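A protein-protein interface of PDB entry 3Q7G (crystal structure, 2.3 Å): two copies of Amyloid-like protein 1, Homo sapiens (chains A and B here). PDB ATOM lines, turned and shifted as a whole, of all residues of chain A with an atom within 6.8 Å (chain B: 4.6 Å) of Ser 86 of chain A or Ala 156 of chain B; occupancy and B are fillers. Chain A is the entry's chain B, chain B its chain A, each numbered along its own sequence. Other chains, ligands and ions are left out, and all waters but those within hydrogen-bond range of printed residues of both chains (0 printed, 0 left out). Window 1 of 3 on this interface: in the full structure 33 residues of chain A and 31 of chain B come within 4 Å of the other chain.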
ATOM      1  N   LEU A  81      35.577  15.102   3.442  1.00  0.00           N
ATOM      2  CA  LEU A  81      35.469  13.753   2.929  1.00  0.00           C
ATOM      3  C   LEU A  81      34.649  12.856   3.859  1.00  0.00           C
ATOM      4  O   LEU A  81      33.797  12.107   3.394  1.00  0.00           O
ATOM      5  CB  LEU A  81      36.854  13.174   2.717  1.00  0.00           C
ATOM      6  CG  LEU A  81      36.920  12.007   1.753  1.00  0.00           C
ATOM      7  CD1 LEU A  81      36.202  12.360   0.478  1.00  0.00           C
ATOM      8  CD2 LEU A  81      38.370  11.685   1.488  1.00  0.00           C
ATOM      9  N   GLU A  82      34.907  12.925   5.162  1.00  0.00           N
ATOM     10  CA  GLU A  82      34.155  12.112   6.116  1.00  0.00           C
ATOM     11  C   GLU A  82      32.651  12.421   6.037  1.00  0.00           C
ATOM     12  O   GLU A  82      31.820  11.527   6.170  1.00  0.00           O
ATOM     13  CB  GLU A  82      34.619  12.373   7.547  1.00  0.00           C
ATOM     14  CG  GLU A  82      36.086  12.111   7.802  1.00  0.00           C
ATOM     15  CD  GLU A  82      36.555  12.657   9.148  1.00  0.00           C
ATOM     16  OE1 GLU A  82      35.939  13.626   9.653  1.00  0.00           O
ATOM     17  OE2 GLU A  82      37.556  12.127   9.690  1.00  0.00           O
ATOM     18  N   GLU A  83      32.317  13.692   5.839  1.00  0.00           N
ATOM     19  CA  GLU A  83      30.923  14.111   5.752  1.00  0.00           C
ATOM     20  C   GLU A  83      30.296  13.653   4.439  1.00  0.00           C
ATOM     21  O   GLU A  83      29.111  13.314   4.394  1.00  0.00           O
ATOM     22  CB  GLU A  83      30.823  15.630   5.926  1.00  0.00           C
ATOM     23  CG  GLU A  83      31.035  16.063   7.374  1.00  0.00           C
ATOM     24  CD  GLU A  83      31.380  17.533   7.530  1.00  0.00           C
ATOM     25  OE1 GLU A  83      31.001  18.334   6.640  1.00  0.00           O
ATOM     26  OE2 GLU A  83      32.017  17.885   8.545  1.00  0.00           O
ATOM     27  N   GLN A  84      31.093  13.646   3.376  1.00  0.00           N
ATOM     28  CA  GLN A  84      30.625  13.167   2.084  1.00  0.00           C
ATOM     29  C   GLN A  84      30.356  11.667   2.254  1.00  0.00           C
ATOM     30  O   GLN A  84      29.358  11.135   1.755  1.00  0.00           O
ATOM     31  CB  GLN A  84      31.705  13.352   1.018  1.00  0.00           C
ATOM     32  CG  GLN A  84      31.606  14.616   0.200  1.00  0.00           C
ATOM     33  CD  GLN A  84      32.882  14.889  -0.578  1.00  0.00           C
ATOM     34  OE1 GLN A  84      33.563  13.964  -1.030  1.00  0.00           O
ATOM     35  NE2 GLN A  84      33.210  16.166  -0.745  1.00  0.00           N
ATOM     36  N   VAL A  85      31.248  10.989   2.971  1.00  0.00           N
ATOM     37  CA  VAL A  85      31.116   9.556   3.199  1.00  0.00           C
ATOM     38  C   VAL A  85      29.818   9.222   3.945  1.00  0.00           C
ATOM     39  O   VAL A  85      29.043   8.367   3.517  1.00  0.00           O
ATOM     40  CB  VAL A  85      32.336   9.001   3.985  1.00  0.00           C
ATOM     41  CG1 VAL A  85      31.997   7.656   4.579  1.00  0.00           C
ATOM     42  CG2 VAL A  85      33.561   8.876   3.045  1.00  0.00           C
ATOM     43  N   SER A  86      29.591   9.907   5.055  1.00  0.00           N
ATOM     44  CA  SER A  86      28.398   9.701   5.866  1.00  0.00           C
ATOM     45  C   SER A  86      27.104   9.879   5.063  1.00  0.00           C
ATOM     46  O   SER A  86      26.220   9.019   5.092  1.00  0.00           O
ATOM     47  CB  SER A  86      28.405  10.687   7.035  1.00  0.00           C
ATOM     48  OG  SER A  86      27.290  10.479   7.885  1.00  0.00           O
ATOM     49  N   GLY A  87      26.996  10.996   4.351  1.00  0.00           N
ATOM     50  CA  GLY A  87      25.802  11.266   3.566  1.00  0.00           C
ATOM     51  C   GLY A  87      25.505  10.174   2.559  1.00  0.00           C
ATOM     52  O   GLY A  87      24.372   9.697   2.433  1.00  0.00           O
ATOM     53  N   GLU A  88      26.549   9.785   1.839  1.00  0.00           N
ATOM     54  CA  GLU A  88      26.502   8.748   0.812  1.00  0.00           C
ATOM     55  C   GLU A  88      25.986   7.422   1.387  1.00  0.00           C
ATOM     56  O   GLU A  88      25.119   6.759   0.801  1.00  0.00           O
ATOM     57  CB  GLU A  88      27.914   8.573   0.263  1.00  0.00           C
ATOM     58  CG  GLU A  88      28.024   7.853  -1.045  1.00  0.00           C
ATOM     59  CD  GLU A  88      29.384   8.086  -1.678  1.00  0.00           C
ATOM     60  OE1 GLU A  88      30.405   7.826  -1.004  1.00  0.00           O
ATOM     61  OE2 GLU A  88      29.430   8.535  -2.847  1.00  0.00           O
ATOM     62  N   ARG A  89      26.524   7.043   2.539  1.00  0.00           N
ATOM     63  CA  ARG A  89      26.124   5.808   3.200  1.00  0.00           C
ATOM     64  C   ARG A  89      24.648   5.876   3.597  1.00  0.00           C
ATOM     65  O   ARG A  89      23.865   5.008   3.238  1.00  0.00           O
ATOM     66  CB  ARG A  89      26.995   5.545   4.430  1.00  0.00           C
ATOM     67  N   GLN A  90      24.307   6.924   4.343  1.00  0.00           N
ATOM     68  CA  GLN A  90      22.954   7.185   4.832  1.00  0.00           C
ATOM     69  C   GLN A  90      21.933   7.097   3.694  1.00  0.00           C
ATOM     70  O   GLN A  90      20.855   6.533   3.849  1.00  0.00           O
ATOM     71  CB  GLN A  90      22.914   8.580   5.465  1.00  0.00           C
ATOM     72  CG  GLN A  90      21.623   8.946   6.158  1.00  0.00           C
ATOM     73  CD  GLN A  90      21.733  10.271   6.900  1.00  0.00           C
ATOM     74  OE1 GLN A  90      22.550  10.415   7.815  1.00  0.00           O
ATOM     75  NE2 GLN A  90      20.915  11.246   6.507  1.00  0.00           N
ATOM     76  N   ARG A  91      22.278   7.656   2.547  1.00  0.00           N
ATOM     77  CA  ARG A  91      21.373   7.613   1.417  1.00  0.00           C
ATOM     78  C   ARG A  91      21.211   6.169   0.928  1.00  0.00           C
ATOM     79  O   ARG A  91      20.095   5.681   0.771  1.00  0.00           O
ATOM     80  CB  ARG A  91      21.913   8.477   0.300  1.00  0.00           C
ATOM     81  CG  ARG A  91      20.957   8.665  -0.828  1.00  0.00           C
ATOM     82  CD  ARG A  91      21.687   9.186  -2.023  1.00  0.00           C
ATOM     83  NE  ARG A  91      20.787   9.426  -3.137  1.00  0.00           N
ATOM     84  CZ  ARG A  91      21.182   9.522  -4.397  1.00  0.00           C
ATOM     85  NH1 ARG A  91      22.467   9.387  -4.700  1.00  0.00           N
ATOM     86  NH2 ARG A  91      20.288   9.777  -5.343  1.00  0.00           N
ATOM     87  N   GLN B 152      36.918   4.414   7.457  1.00  0.00           N
ATOM     88  CA  GLN B 152      35.836   4.708   6.533  1.00  0.00           C
ATOM     89  C   GLN B 152      34.436   4.383   7.087  1.00  0.00           C
ATOM     90  O   GLN B 152      33.502   5.160   6.881  1.00  0.00           O
ATOM     91  CB  GLN B 152      36.091   3.951   5.229  1.00  0.00           C
ATOM     92  CG  GLN B 152      34.988   4.031   4.232  1.00  0.00           C
ATOM     93  CD  GLN B 152      33.987   2.884   4.347  1.00  0.00           C
ATOM     94  OE1 GLN B 152      32.864   2.990   3.876  1.00  0.00           O
ATOM     95  NE2 GLN B 152      34.418   1.779   4.959  1.00  0.00           N
ATOM     96  N   HIS B 153      34.280   3.273   7.816  1.00  0.00           N
ATOM     97  CA  HIS B 153      32.957   2.952   8.372  1.00  0.00           C
ATOM     98  C   HIS B 153      32.633   3.826   9.589  1.00  0.00           C
ATOM     99  O   HIS B 153      31.474   4.182   9.786  1.00  0.00           O
ATOM    100  CB  HIS B 153      32.831   1.471   8.748  1.00  0.00           C
ATOM    101  CG  HIS B 153      31.416   1.067   9.070  1.00  0.00           C
ATOM    102  ND1 HIS B 153      31.010   0.721  10.351  1.00  0.00           N
ATOM    103  CD2 HIS B 153      30.305   1.036   8.293  1.00  0.00           C
ATOM    104  CE1 HIS B 153      29.715   0.494  10.344  1.00  0.00           C
ATOM    105  NE2 HIS B 153      29.269   0.679   9.112  1.00  0.00           N
ATOM    106  N   VAL B 154      33.636   4.146  10.406  1.00  0.00           N
ATOM    107  CA  VAL B 154      33.430   5.000  11.576  1.00  0.00           C
ATOM    108  C   VAL B 154      32.897   6.371  11.138  1.00  0.00           C
ATOM    109  O   VAL B 154      32.065   6.985  11.813  1.00  0.00           O
ATOM    110  CB  VAL B 154      34.767   5.257  12.340  1.00  0.00           C
ATOM    111  CG1 VAL B 154      34.513   6.209  13.524  1.00  0.00           C
ATOM    112  CG2 VAL B 154      35.361   3.949  12.826  1.00  0.00           C
ATOM    113  N   ALA B 155      33.392   6.838  10.000  1.00  0.00           N
ATOM    114  CA  ALA B 155      33.011   8.126   9.456  1.00  0.00           C
ATOM    115  C   ALA B 155      31.516   8.252   9.185  1.00  0.00           C
ATOM    116  O   ALA B 155      30.968   9.354   9.214  1.00  0.00           O
ATOM    117  CB  ALA B 155      33.792   8.400   8.163  1.00  0.00           C
ATOM    118  N   ALA B 156      30.851   7.132   8.928  1.00  0.00           N
ATOM    119  CA  ALA B 156      29.418   7.155   8.658  1.00  0.00           C
ATOM    120  C   ALA B 156      28.591   6.929   9.918  1.00  0.00           C
ATOM    121  O   ALA B 156      27.471   7.441  10.033  1.00  0.00           O
ATOM    122  CB  ALA B 156      29.070   6.105   7.611  1.00  0.00           C
ATOM    123  N   VAL B 157      29.149   6.170  10.856  1.00  0.00           N
ATOM    124  CA  VAL B 157      28.456   5.844  12.093  1.00  0.00           C
ATOM    125  C   VAL B 157      28.534   6.943  13.147  1.00  0.00           C
ATOM    126  O   VAL B 157      27.508   7.465  13.595  1.00  0.00           O
ATOM    127  CB  VAL B 157      29.023   4.536  12.680  1.00  0.00           C
ATOM    128  N   ASP B 158      29.755   7.293  13.537  1.00  0.00           N
ATOM    129  CA  ASP B 158      29.969   8.325  14.541  1.00  0.00           C
ATOM    130  C   ASP B 158      31.031   9.315  14.078  1.00  0.00           C
ATOM    131  O   ASP B 158      32.206   9.209  14.437  1.00  0.00           O
ATOM    132  CB  ASP B 158      30.373   7.675  15.869  1.00  0.00           C
ATOM    133  CG  ASP B 158      30.682   8.691  16.952  1.00  0.00           C
ATOM    134  OD1 ASP B 158      30.093   9.798  16.924  1.00  0.00           O
ATOM    135  OD2 ASP B 158      31.507   8.382  17.837  1.00  0.00           O
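O of Glu 82 of chain A touches O of Ala 155 of chain B (3.8 Å).
Gln 152 of chain B touches Val 85 of chain A (O to CG1, 3.7 Å).
Ser 86 of chain A touches Ala 155 of chain B.
Ser 86 of chain A touches Ala 156 of chain B (OG to O, 3.7 Å).
Arg 89 of chain A touches Ala 156 of chain B (CB to CB, 3.8 Å).
No position is printed for both chains.
Of the 5 pairs that touch across the chains among the printed residues, none has its exchanged pair printed and touching as well.
Ser 86 of chain A touches two residues of chain B.
Of chain A, only Ser 86 and Arg 89 come within 4 Å of Ala 156 of chain B.
Of the printed residues of chain B, Glu 82 of chain A touches Ala 155.
Of the printed residues of chain B, Val 85 of chain A touches Gln 152.
Printed residues of chain A within 4 Å of Ala 155 of chain B: Glu 82 (3.8 Å) and Ser 86 (3.6 Å).
Of the printed residues of chain A, Gln 152 of chain B touches Val 85.
Gln 84 of chain A touches none of the printed residues of chain B.
Arg 91 of chain A touches none of the printed residues of chain B.
The nearest printed residue of chain B that does not touch Val 85 of chain A is Ala 155 of chain B (4.1 Å).
Of the 7 printed residues of chain B, 3 touch a printed residue of chain A.
Hydrophobic or aromatic side chains of chain B that line the printed part of chain A: Ala 156.
Of the 11 printed residues of chain A, 4 touch a printed residue of chain B.
Printed residues of chain A that touch a printed residue of chain B: Glu 82, Val 85, Ser 86 and Arg 89.
Hydrophobic or aromatic side chains of chain A that line the printed part of chain B: Val 85.
Along chain A the printed residues that touch a printed residue of chain B span positions 82 to 89.
Among the printed residues, no Asp or Glu carboxylate lies within 4 Å of a Lys or Arg side-chain nitrogen of the other chain.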
